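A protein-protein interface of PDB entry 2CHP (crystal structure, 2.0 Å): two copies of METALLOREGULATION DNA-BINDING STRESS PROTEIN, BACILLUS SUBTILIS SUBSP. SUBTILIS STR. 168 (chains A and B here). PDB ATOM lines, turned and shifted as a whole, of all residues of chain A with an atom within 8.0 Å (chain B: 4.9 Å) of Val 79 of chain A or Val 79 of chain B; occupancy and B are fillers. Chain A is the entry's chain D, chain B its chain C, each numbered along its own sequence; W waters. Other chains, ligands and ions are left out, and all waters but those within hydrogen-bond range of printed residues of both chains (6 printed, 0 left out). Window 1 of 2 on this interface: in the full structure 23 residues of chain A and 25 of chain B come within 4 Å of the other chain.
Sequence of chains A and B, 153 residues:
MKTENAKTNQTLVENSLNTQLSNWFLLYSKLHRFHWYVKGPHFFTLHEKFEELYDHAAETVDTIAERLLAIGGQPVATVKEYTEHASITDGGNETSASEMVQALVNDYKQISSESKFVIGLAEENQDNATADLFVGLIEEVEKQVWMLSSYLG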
ATOM      1  N   SER A  22      27.304   8.810 -11.143  1.00  0.00           N
ATOM      2  CA  SER A  22      26.362   9.850 -10.752  1.00  0.00           C
ATOM      3  C   SER A  22      26.787  10.622  -9.495  1.00  0.00           C
ATOM      4  O   SER A  22      26.608  11.859  -9.444  1.00  0.00           O
ATOM      5  CB  SER A  22      24.928   9.291 -10.614  1.00  0.00           C
ATOM      6  OG  SER A  22      24.491   8.741 -11.841  1.00  0.00           O
ATOM      7  N   PHE A  25      29.676  13.030 -10.267  1.00  0.00           N
ATOM      8  CA  PHE A  25      29.243  14.225 -10.955  1.00  0.00           C
ATOM      9  C   PHE A  25      28.494  15.210 -10.046  1.00  0.00           C
ATOM     10  O   PHE A  25      28.694  16.459 -10.109  1.00  0.00           O
ATOM     11  CB  PHE A  25      28.436  13.889 -12.198  1.00  0.00           C
ATOM     12  CG  PHE A  25      28.387  15.005 -13.202  1.00  0.00           C
ATOM     13  CD1 PHE A  25      29.202  14.991 -14.326  1.00  0.00           C
ATOM     14  CD2 PHE A  25      27.504  16.082 -13.038  1.00  0.00           C
ATOM     15  CE1 PHE A  25      29.158  16.059 -15.214  1.00  0.00           C
ATOM     16  CE2 PHE A  25      27.452  17.123 -13.942  1.00  0.00           C
ATOM     17  CZ  PHE A  25      28.272  17.097 -15.008  1.00  0.00           C
ATOM     18  N   LEU A  26      27.674  14.677  -9.159  1.00  0.00           N
ATOM     19  CA  LEU A  26      26.993  15.533  -8.207  1.00  0.00           C
ATOM     20  C   LEU A  26      27.934  16.165  -7.164  1.00  0.00           C
ATOM     21  O   LEU A  26      27.727  17.310  -6.760  1.00  0.00           O
ATOM     22  CB  LEU A  26      25.845  14.791  -7.545  1.00  0.00           C
ATOM     23  CG  LEU A  26      24.660  14.413  -8.459  1.00  0.00           C
ATOM     24  CD1 LEU A  26      23.430  13.966  -7.555  1.00  0.00           C
ATOM     25  CD2 LEU A  26      24.220  15.543  -9.414  1.00  0.00           C
ATOM     26  N   LEU A  27      28.961  15.430  -6.786  1.00  0.00           N
ATOM     27  CA  LEU A  27      29.986  15.956  -5.904  1.00  0.00           C
ATOM     28  C   LEU A  27      30.740  17.101  -6.608  1.00  0.00           C
ATOM     29  O   LEU A  27      31.079  18.091  -5.956  1.00  0.00           O
ATOM     30  CB  LEU A  27      30.925  14.856  -5.406  1.00  0.00           C
ATOM     31  CG  LEU A  27      31.901  15.231  -4.283  1.00  0.00           C
ATOM     32  CD1 LEU A  27      31.107  15.639  -3.002  1.00  0.00           C
ATOM     33  CD2 LEU A  27      32.942  14.143  -3.955  1.00  0.00           C
ATOM     34  N   TYR A  28      31.147  16.899  -7.880  1.00  0.00           N
ATOM     35  CA  TYR A  28      31.730  17.975  -8.690  1.00  0.00           C
ATOM     36  C   TYR A  28      30.898  19.258  -8.598  1.00  0.00           C
ATOM     37  O   TYR A  28      31.410  20.376  -8.352  1.00  0.00           O
ATOM     38  CB  TYR A  28      31.791  17.473 -10.146  1.00  0.00           C
ATOM     39  CG  TYR A  28      32.363  18.460 -11.149  1.00  0.00           C
ATOM     40  CD1 TYR A  28      31.519  19.205 -11.955  1.00  0.00           C
ATOM     41  CD2 TYR A  28      33.744  18.593 -11.327  1.00  0.00           C
ATOM     42  CE1 TYR A  28      32.030  20.129 -12.892  1.00  0.00           C
ATOM     43  CE2 TYR A  28      34.271  19.538 -12.243  1.00  0.00           C
ATOM     44  CZ  TYR A  28      33.392  20.289 -13.017  1.00  0.00           C
ATOM     45  OH  TYR A  28      33.876  21.181 -13.959  1.00  0.00           O
ATOM     46  N   SER A  29      29.598  19.117  -8.780  1.00  0.00           N
ATOM     47  CA  SER A  29      28.621  20.253  -8.632  1.00  0.00           C
ATOM     48  C   SER A  29      28.653  20.933  -7.248  1.00  0.00           C
ATOM     49  O   SER A  29      28.819  22.182  -7.140  1.00  0.00           O
ATOM     50  CB  SER A  29      27.226  19.779  -9.001  1.00  0.00           C
ATOM     51  OG  SER A  29      26.261  20.811  -8.831  1.00  0.00           O
ATOM     52  N   LYS A  30      28.586  20.115  -6.168  1.00  0.00           N
ATOM     53  CA  LYS A  30      28.547  20.604  -4.804  1.00  0.00           C
ATOM     54  C   LYS A  30      29.819  21.309  -4.479  1.00  0.00           C
ATOM     55  O   LYS A  30      29.769  22.337  -3.852  1.00  0.00           O
ATOM     56  CB  LYS A  30      28.324  19.439  -3.834  1.00  0.00           C
ATOM     57  CG  LYS A  30      28.071  19.833  -2.392  1.00  0.00           C
ATOM     58  CD  LYS A  30      27.894  18.619  -1.435  1.00  0.00           C
ATOM     59  CE  LYS A  30      26.662  17.796  -1.722  1.00  0.00           C
ATOM     60  NZ  LYS A  30      26.258  16.835  -0.594  1.00  0.00           N
ATOM     61  N   VAL A  76      25.350   6.572 -17.847  1.00  0.00           N
ATOM     62  CA  VAL A  76      24.466   7.702 -17.767  1.00  0.00           C
ATOM     63  C   VAL A  76      25.264   8.966 -18.017  1.00  0.00           C
ATOM     64  O   VAL A  76      26.461   8.984 -17.764  1.00  0.00           O
ATOM     65  CB  VAL A  76      23.681   7.732 -16.378  1.00  0.00           C
ATOM     66  CG1 VAL A  76      22.721   6.549 -16.304  1.00  0.00           C
ATOM     67  CG2 VAL A  76      24.591   7.846 -15.204  1.00  0.00           C
ATOM     68  N   ALA A  77      24.604  10.005 -18.535  1.00  0.00           N
ATOM     69  CA  ALA A  77      25.291  11.145 -19.119  1.00  0.00           C
ATOM     70  C   ALA A  77      24.407  12.375 -19.311  1.00  0.00           C
ATOM     71  O   ALA A  77      24.668  13.177 -20.237  1.00  0.00           O
ATOM     72  CB  ALA A  77      25.927  10.775 -20.421  1.00  0.00           C
ATOM     73  N   THR A  78      23.376  12.524 -18.453  1.00  0.00           N
ATOM     74  CA  THR A  78      22.611  13.745 -18.364  1.00  0.00           C
ATOM     75  C   THR A  78      22.381  14.040 -16.891  1.00  0.00           C
ATOM     76  O   THR A  78      22.434  13.111 -16.070  1.00  0.00           O
ATOM     77  CB  THR A  78      21.258  13.661 -19.010  1.00  0.00           C
ATOM     78  OG1 THR A  78      20.478  12.642 -18.358  1.00  0.00           O
ATOM     79  CG2 THR A  78      21.377  13.343 -20.518  1.00  0.00           C
ATOM     80  N   VAL A  79      22.170  15.323 -16.534  1.00  0.00           N
ATOM     81  CA  VAL A  79      22.001  15.666 -15.119  1.00  0.00           C
ATOM     82  C   VAL A  79      20.706  15.056 -14.519  1.00  0.00           C
ATOM     83  O   VAL A  79      20.639  14.795 -13.290  1.00  0.00           O
ATOM     84  CB  VAL A  79      22.139  17.199 -14.801  1.00  0.00           C
ATOM     85  CG1 VAL A  79      23.569  17.740 -15.130  1.00  0.00           C
ATOM     86  CG2 VAL A  79      21.072  18.068 -15.530  1.00  0.00           C
ATOM     87  N   LYS A  80      19.708  14.808 -15.363  1.00  0.00           N
ATOM     88  CA  LYS A  80      18.439  14.200 -14.898  1.00  0.00           C
ATOM     89  C   LYS A  80      18.758  12.751 -14.509  1.00  0.00           C
ATOM     90  O   LYS A  80      18.350  12.296 -13.472  1.00  0.00           O
ATOM     91  CB  LYS A  80      17.362  14.252 -15.985  1.00  0.00           C
ATOM     92  CG  LYS A  80      16.023  13.569 -15.667  1.00  0.00           C
ATOM     93  CD  LYS A  80      15.121  13.588 -16.943  1.00  0.00           C
ATOM     94  CE  LYS A  80      13.750  12.862 -16.740  1.00  0.00           C
ATOM     95  NZ  LYS A  80      13.095  13.403 -15.499  1.00  0.00           N
ATOM     96  N   GLU A  81      19.492  12.034 -15.339  1.00  0.00           N
ATOM     97  CA  GLU A  81      20.006  10.689 -14.983  1.00  0.00           C
ATOM     98  C   GLU A  81      20.897  10.654 -13.785  1.00  0.00           C
ATOM     99  O   GLU A  81      20.749   9.775 -12.942  1.00  0.00           O
ATOM    100  CB  GLU A  81      20.750  10.039 -16.156  1.00  0.00           C
ATOM    101  CG  GLU A  81      19.777   9.559 -17.291  1.00  0.00           C
ATOM    102  CD  GLU A  81      20.533   9.122 -18.550  1.00  0.00           C
ATOM    103  OE1 GLU A  81      21.537   9.827 -18.961  1.00  0.00           O
ATOM    104  OE2 GLU A  81      20.168   8.049 -19.113  1.00  0.00           O
ATOM    105  N   TYR A  82      21.827  11.616 -13.647  1.00  0.00           N
ATOM    106  CA  TYR A  82      22.646  11.628 -12.427  1.00  0.00           C
ATOM    107  C   TYR A  82      21.779  11.801 -11.185  1.00  0.00           C
ATOM    108  O   TYR A  82      22.043  11.173 -10.179  1.00  0.00           O
ATOM    109  CB  TYR A  82      23.740  12.721 -12.429  1.00  0.00           C
ATOM    110  CG  TYR A  82      24.691  12.635 -13.578  1.00  0.00           C
ATOM    111  CD1 TYR A  82      25.192  11.392 -14.024  1.00  0.00           C
ATOM    112  CD2 TYR A  82      25.126  13.777 -14.212  1.00  0.00           C
ATOM    113  CE1 TYR A  82      26.149  11.300 -15.062  1.00  0.00           C
ATOM    114  CE2 TYR A  82      26.032  13.705 -15.330  1.00  0.00           C
ATOM    115  CZ  TYR A  82      26.563  12.474 -15.716  1.00  0.00           C
ATOM    116  OH  TYR A  82      27.463  12.431 -16.792  1.00  0.00           O
ATOM    117  N   THR A  83      20.824  12.717 -11.216  1.00  0.00           N
ATOM    118  CA  THR A  83      19.924  12.934 -10.044  1.00  0.00           C
ATOM    119  C   THR A  83      19.174  11.591  -9.718  1.00  0.00           C
ATOM    120  O   THR A  83      19.084  11.162  -8.555  1.00  0.00           O
ATOM    121  CB  THR A  83      18.939  14.151 -10.303  1.00  0.00           C
ATOM    122  OG1 THR A  83      19.686  15.357 -10.644  1.00  0.00           O
ATOM    123  CG2 THR A  83      17.985  14.448  -9.054  1.00  0.00           C
ATOM    124  N   GLU A  84      18.653  10.962 -10.783  1.00  0.00           N
ATOM    125  CA  GLU A  84      17.884   9.680 -10.729  1.00  0.00           C
ATOM    126  C   GLU A  84      18.663   8.434 -10.264  1.00  0.00           C
ATOM    127  O   GLU A  84      18.064   7.529  -9.721  1.00  0.00           O
ATOM    128  CB  GLU A  84      17.167   9.416 -12.067  1.00  0.00           C
ATOM    129  CG  GLU A  84      16.050  10.486 -12.202  1.00  0.00           C
ATOM    130  CD  GLU A  84      15.094  10.340 -13.376  1.00  0.00           C
ATOM    131  OE1 GLU A  84      15.327   9.474 -14.219  1.00  0.00           O
ATOM    132  OE2 GLU A  84      14.139  11.213 -13.421  1.00  0.00           O
ATOM    133  N   HIS A  85      19.986   8.428 -10.418  1.00  0.00           N
ATOM    134  CA  HIS A  85      20.809   7.235 -10.159  1.00  0.00           C
ATOM    135  C   HIS A  85      21.770   7.357  -8.960  1.00  0.00           C
ATOM    136  O   HIS A  85      22.284   6.357  -8.462  1.00  0.00           O
ATOM    137  CB  HIS A  85      21.616   6.949 -11.421  1.00  0.00           C
ATOM    138  CG  HIS A  85      20.787   6.385 -12.556  1.00  0.00           C
ATOM    139  ND1 HIS A  85      20.738   5.034 -12.821  1.00  0.00           N
ATOM    140  CD2 HIS A  85      19.952   6.974 -13.455  1.00  0.00           C
ATOM    141  CE1 HIS A  85      19.935   4.819 -13.852  1.00  0.00           C
ATOM    142  NE2 HIS A  85      19.437   5.971 -14.253  1.00  0.00           N
ATOM    143  N   ALA A  86      22.055   8.584  -8.542  1.00  0.00           N
ATOM    144  CA  ALA A  86      22.956   8.867  -7.431  1.00  0.00           C
ATOM    145  C   ALA A  86      22.331   8.471  -6.071  1.00  0.00           C
ATOM    146  O   ALA A  86      21.083   8.478  -5.935  1.00  0.00           O
ATOM    147  CB  ALA A  86      23.286  10.341  -7.416  1.00  0.00           C
ATOM    148  N   THR A  89      23.349  13.722  -2.848  1.00  0.00           N
ATOM    149  CA  THR A  89      22.752  14.863  -3.581  1.00  0.00           C
ATOM    150  C   THR A  89      23.736  16.042  -3.685  1.00  0.00           C
ATOM    151  O   THR A  89      24.631  16.147  -2.883  1.00  0.00           O
ATOM    152  CB  THR A  89      21.407  15.321  -2.927  1.00  0.00           C
ATOM    153  OG1 THR A  89      20.797  16.357  -3.720  1.00  0.00           O
ATOM    154  CG2 THR A  89      21.590  15.781  -1.414  1.00  0.00           C
ATOM    155  N   ASP A  90      23.548  16.915  -4.665  1.00  0.00           N
ATOM    156  CA  ASP A  90      24.312  18.178  -4.650  1.00  0.00           C
ATOM    157  C   ASP A  90      23.541  19.283  -3.927  1.00  0.00           C
ATOM    158  O   ASP A  90      24.047  20.382  -3.772  1.00  0.00           O
ATOM    159  CB  ASP A  90      24.717  18.612  -6.096  1.00  0.00           C
ATOM    160  CG  ASP A  90      23.545  19.009  -6.970  1.00  0.00           C
ATOM    161  OD1 ASP A  90      22.423  18.516  -6.741  1.00  0.00           O
ATOM    162  OD2 ASP A  90      23.758  19.751  -7.959  1.00  0.00           O
ATOM    163  N   GLY A  91      22.308  18.989  -3.476  1.00  0.00           N
ATOM    164  CA  GLY A  91      21.530  19.959  -2.730  1.00  0.00           C
ATOM    165  C   GLY A  91      22.064  20.098  -1.318  1.00  0.00           C
ATOM    166  O   GLY A  91      22.982  19.391  -0.911  1.00  0.00           O
ATOM    167  N   PHE B  25      27.192  25.033 -17.838  1.00  0.00           N
ATOM    168  CA  PHE B  25      27.229  23.757 -17.091  1.00  0.00           C
ATOM    169  C   PHE B  25      26.492  22.659 -17.861  1.00  0.00           C
ATOM    170  O   PHE B  25      26.926  21.495 -17.919  1.00  0.00           O
ATOM    171  CB  PHE B  25      26.679  23.918 -15.694  1.00  0.00           C
ATOM    172  CG  PHE B  25      27.162  22.875 -14.746  1.00  0.00           C
ATOM    173  CD1 PHE B  25      28.187  23.126 -13.877  1.00  0.00           C
ATOM    174  CD2 PHE B  25      26.609  21.611 -14.753  1.00  0.00           C
ATOM    175  CE1 PHE B  25      28.642  22.111 -13.010  1.00  0.00           C
ATOM    176  CE2 PHE B  25      27.040  20.621 -13.883  1.00  0.00           C
ATOM    177  CZ  PHE B  25      28.072  20.880 -13.028  1.00  0.00           C
ATOM    178  N   LEU B  26      25.362  22.984 -18.465  1.00  0.00           N
ATOM    179  CA  LEU B  26      24.641  21.910 -19.208  1.00  0.00           C
ATOM    180  C   LEU B  26      25.376  21.498 -20.499  1.00  0.00           C
ATOM    181  O   LEU B  26      25.314  20.311 -20.941  1.00  0.00           O
ATOM    182  CB  LEU B  26      23.207  22.342 -19.501  1.00  0.00           C
ATOM    183  CG  LEU B  26      22.208  22.477 -18.326  1.00  0.00           C
ATOM    184  CD1 LEU B  26      20.786  22.629 -18.910  1.00  0.00           C
ATOM    185  CD2 LEU B  26      22.239  21.311 -17.351  1.00  0.00           C
ATOM    186  N   SER B  29      28.088  19.059 -19.424  1.00  0.00           N
ATOM    187  CA  SER B  29      27.414  17.730 -19.351  1.00  0.00           C
ATOM    188  C   SER B  29      27.229  17.056 -20.756  1.00  0.00           C
ATOM    189  O   SER B  29      27.653  15.894 -20.954  1.00  0.00           O
ATOM    190  CB  SER B  29      26.092  17.858 -18.571  1.00  0.00           C
ATOM    191  OG  SER B  29      25.344  16.657 -18.513  1.00  0.00           O
ATOM    192  N   ALA B  77      23.876  27.103  -8.296  1.00  0.00           N
ATOM    193  CA  ALA B  77      24.949  26.141  -7.972  1.00  0.00           C
ATOM    194  C   ALA B  77      24.481  24.672  -7.649  1.00  0.00           C
ATOM    195  O   ALA B  77      25.131  23.892  -6.885  1.00  0.00           O
ATOM    196  CB  ALA B  77      25.939  26.759  -6.881  1.00  0.00           C
ATOM    197  N   THR B  78      23.371  24.283  -8.281  1.00  0.00           N
ATOM    198  CA  THR B  78      22.866  22.891  -8.248  1.00  0.00           C
ATOM    199  C   THR B  78      22.344  22.506  -9.616  1.00  0.00           C
ATOM    200  O   THR B  78      21.883  23.380 -10.365  1.00  0.00           O
ATOM    201  CB  THR B  78      21.731  22.693  -7.237  1.00  0.00           C
ATOM    202  OG1 THR B  78      20.615  23.562  -7.576  1.00  0.00           O
ATOM    203  CG2 THR B  78      22.231  23.059  -5.833  1.00  0.00           C
ATOM    204  N   VAL B  79      22.374  21.209  -9.930  1.00  0.00           N
ATOM    205  CA  VAL B  79      21.925  20.745 -11.259  1.00  0.00           C
ATOM    206  C   VAL B  79      20.419  21.015 -11.508  1.00  0.00           C
ATOM    207  O   VAL B  79      20.018  21.347 -12.630  1.00  0.00           O
ATOM    208  CB  VAL B  79      22.334  19.294 -11.558  1.00  0.00           C
ATOM    209  CG1 VAL B  79      23.959  19.181 -11.557  1.00  0.00           C
ATOM    210  CG2 VAL B  79      21.559  18.322 -10.541  1.00  0.00           C
ATOM    211  N   LYS B  80      19.627  20.975 -10.449  1.00  0.00           N
ATOM    212  CA  LYS B  80      18.197  21.375 -10.523  1.00  0.00           C
ATOM    213  C   LYS B  80      18.019  22.826 -10.974  1.00  0.00           C
ATOM    214  O   LYS B  80      17.253  23.097 -11.878  1.00  0.00           O
ATOM    215  CB  LYS B  80      17.440  21.121  -9.190  1.00  0.00           C
ATOM    216  CG  LYS B  80      15.971  21.524  -9.272  1.00  0.00           C
ATOM    217  CD  LYS B  80      15.161  21.142  -8.003  1.00  0.00           C
ATOM    218  CE  LYS B  80      13.630  21.416  -8.265  1.00  0.00           C
ATOM    219  NZ  LYS B  80      12.791  20.864  -7.230  1.00  0.00           N
ATOM    220  N   GLU B  81      18.781  23.740 -10.387  1.00  0.00           N
ATOM    221  CA  GLU B  81      18.767  25.166 -10.774  1.00  0.00           C
ATOM    222  C   GLU B  81      19.306  25.381 -12.197  1.00  0.00           C
ATOM    223  O   GLU B  81      18.711  26.126 -12.953  1.00  0.00           O
ATOM    224  CB  GLU B  81      19.557  26.002  -9.739  1.00  0.00           C
ATOM    225  CG  GLU B  81      18.860  26.188  -8.385  1.00  0.00           C
ATOM    226  CD  GLU B  81      19.802  26.854  -7.324  1.00  0.00           C
ATOM    227  OE1 GLU B  81      20.881  26.343  -7.080  1.00  0.00           O
ATOM    228  OE2 GLU B  81      19.440  27.903  -6.764  1.00  0.00           O
ATOM    229  N   TYR B  82      20.368  24.678 -12.587  1.00  0.00           N
ATOM    230  CA  TYR B  82      20.861  24.803 -13.959  1.00  0.00           C
ATOM    231  C   TYR B  82      19.775  24.430 -14.927  1.00  0.00           C
ATOM    232  O   TYR B  82      19.459  25.178 -15.863  1.00  0.00           O
ATOM    233  CB  TYR B  82      22.127  23.924 -14.186  1.00  0.00           C
ATOM    234  CG  TYR B  82      23.352  24.304 -13.296  1.00  0.00           C
ATOM    235  CD1 TYR B  82      23.656  25.610 -13.001  1.00  0.00           C
ATOM    236  CD2 TYR B  82      24.167  23.356 -12.790  1.00  0.00           C
ATOM    237  CE1 TYR B  82      24.765  25.945 -12.175  1.00  0.00           C
ATOM    238  CE2 TYR B  82      25.253  23.678 -11.989  1.00  0.00           C
ATOM    239  CZ  TYR B  82      25.557  24.988 -11.708  1.00  0.00           C
ATOM    240  OH  TYR B  82      26.647  25.320 -10.920  1.00  0.00           O
ATOM    241  N   THR B  83      19.220  23.245 -14.745  1.00  0.00           N
ATOM    242  CA  THR B  83      18.036  22.796 -15.580  1.00  0.00           C
ATOM    243  C   THR B  83      16.963  23.858 -15.690  1.00  0.00           C
ATOM    244  O   THR B  83      16.496  24.152 -16.798  1.00  0.00           O
ATOM    245  CB  THR B  83      17.433  21.494 -15.054  1.00  0.00           C
ATOM    246  OG1 THR B  83      18.441  20.439 -15.065  1.00  0.00           O
ATOM    247  CG2 THR B  83      16.212  21.027 -15.943  1.00  0.00           C
ATOM    248  N   ASP B  90      20.810  19.698 -21.731  1.00  0.00           N
ATOM    249  CA  ASP B  90      21.808  18.630 -21.975  1.00  0.00           C
ATOM    250  C   ASP B  90      21.178  17.345 -22.453  1.00  0.00           C
ATOM    251  O   ASP B  90      21.903  16.388 -22.805  1.00  0.00           O
ATOM    252  CB  ASP B  90      22.774  18.376 -20.770  1.00  0.00           C
ATOM    253  CG  ASP B  90      22.079  17.727 -19.560  1.00  0.00           C
ATOM    254  OD1 ASP B  90      20.854  17.843 -19.474  1.00  0.00           O
ATOM    255  OD2 ASP B  90      22.742  17.076 -18.720  1.00  0.00           O
HETATM  256  O   HOH W   1      25.563  22.148  -5.235  1.00  0.00           O
HETATM  257  O   HOH W   2      27.080  14.448 -18.494  1.00  0.00           O
HETATM  258  O   HOH W   3      20.146  19.695  -7.670  1.00  0.00           O
HETATM  259  O   HOH W   4      19.172  16.257 -18.003  1.00  0.00           O
HETATM  260  O   HOH W   5      27.444  23.272  -9.286  1.00  0.00           O
HETATM  261  O   HOH W   6      24.130  15.160 -22.090  1.00  0.00           O
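Among the printed residues, pairs that only touch across the chains: Asp 90 of chain A with Thr 78 of chain B (3.3 Å), Thr 78 of chain A with Asp 90 of chain B (3.4 Å), Thr 83 of chain A with Val 79 of chain B (3.5 Å), Phe 25 of chain A with Phe 25 of chain B (3.5 Å), Val 79 of chain A with Thr 83 of chain B (3.6 Å), Ser 29 of chain A with Ala 77 of chain B (3.8 Å), Val 79 of chain A with Val 79 of chain B (3.9 Å), Val 79 of chain A with Leu 26 of chain B (3.9 Å), Ser 29 of chain A with Val 79 of chain B (3.9 Å), Tyr 28 of chain A with Phe 25 of chain B (3.9 Å), Ala 77 of chain A with Ser 29 of chain B (3.9 Å), Val 79 of chain A with Ser 29 of chain B (3.97 Å) and Thr 78 of chain A with Ser 29 of chain B (3.996 Å).
Ser 29 of chain A touches Val 79 of chain B, and with the chains exchanged Val 79 of chain A touches Ser 29 of chain B. Thr 78 of chain A touches Ser 29 of chain B, but with the chains exchanged Ser 29 of chain A does not touch Thr 78 of chain B (4.02 Å). Val 79 of chain A touches Leu 26 of chain B, but with the chains exchanged Leu 26 of chain A does not touch Val 79 of chain B (4.01 Å). Val 79 of chain A touches Thr 83 of chain B, and with the chains exchanged Thr 83 of chain A touches Val 79 of chain B. 11 positions are printed for both chains. Of the 15 pairs that touch across the chains among the printed residues, 12 have their exchanged pair printed and touching as well.
The side-chain hydroxyl of Ser 29 of chain B sits at hydrogen-bond distance from the side-chain carboxylate of Asp 90 of chain B, 2.6 Å away. The backbone NH (N) of Ala 77 of chain B is in hydrogen-bond range of the side-chain carboxylate (OE1) of Glu 81 of chain B (3.3 Å). The side-chain hydroxyl of Thr 78 of chain B lies within hydrogen-bond range of the side-chain carboxylate of Glu 81 of chain B (2.8 Å). The side-chain carboxylate of Glu 81 of chain A sits at hydrogen-bond distance from the backbone NH of Ala 77 of chain A (3.1 Å). OG1 of Thr 78 of chain A sits at hydrogen-bond distance from OE1 of Glu 81 of chain A (3.1 Å). The side-chain hydroxyl (OG1) of Thr 83 of chain A lies within hydrogen-bond range of the backbone carbonyl oxygen (O) of Val 79 of chain A, 2.9 Å away.
Of the printed residues of chain B, Ser 29 of chain A touches Ala 77 (3.8 Å) and Val 79 (3.9 Å). Printed residues of chain B within 4 Å of Thr 78 of chain A: Ser 29 and Asp 90. Val 79 of chain A touches just these residues of chain B: Leu 26, Ser 29, Val 79, Thr 83 and Asp 90. Gly 91 of chain A touches none of the printed residues of chain B. Printed residues of chain A within 4 Å of Phe 25 of chain B: Phe 25 and Tyr 28. Of the printed residues of chain A, Val 79 of chain B touches Ser 29, Val 79, Thr 83 and Asp 90. Tyr 82 of chain B touches none of the printed residues of chain A. Printed residues of chain A within 4 Å of Thr 83 of chain B: Val 79 (3.6 Å). Of the printed residues of chain A, Asp 90 of chain B touches Thr 78 (3.4 Å) and Val 79 (2.9 Å). The nearest printed residue of chain A that does not touch Thr 83 of chain B is Lys 80 of chain A (5.8 Å).
N of Val 79 of chain B lies within hydrogen-bond range of OD2 of Asp 90 of chain A. The backbone NH (N) of Val 79 of chain A is in hydrogen-bond range of the side-chain carboxylate (OD2) of Asp 90 of chain B.
Water W1 bridges the backbone carbonyl oxygen of Ala 77 of chain B (2.4 Å) and the backbone carbonyl oxygen of Asp 90 of chain A (2.7 Å). Water W6 bridges O of Asp 90 of chain B and O of Ala 77 of chain A. Water W2 lies within hydrogen-bond range of OH of Tyr 82 of chain A (2.7 Å), OG of Ser 29 of chain B (2.8 Å) and O of Ala 77 of chain A (3.2 Å). Water W3 lies within hydrogen-bond range of the side-chain carboxylate of Asp 90 of chain A (2.7 Å) and the backbone NH of Lys 80 of chain B (3.1 Å). Water W5 lies within hydrogen-bond range of OH of Tyr 82 of chain B, OG of Ser 29 of chain A and O of Ala 77 of chain B. Water W4 lies within hydrogen-bond range of the side-chain carboxylate (OD1) of Asp 90 of chain B (2.7 Å), the backbone NH (N) of Lys 80 of chain A (3.1 Å) and the backbone NH (N) of Val 79 of chain A (3.5 Å).
Hydrophobic or aromatic side chains of chain B that line the printed part of chain A: Phe 25, Leu 26 and Val 79. Printed residues of chain A that touch a printed residue of chain B: Phe 25, Tyr 28, Ser 29, Ala 77, Thr 78, Val 79, Thr 83 and Asp 90. Hydrophobic or aromatic side chains of chain A within 4 Å of the printed part of chain B: Phe 25, Tyr 28 and Val 79. Among the printed residues, no Asp or Glu carboxylate lies within 4 Å of a Lys or Arg side-chain nitrogen of the other chain.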
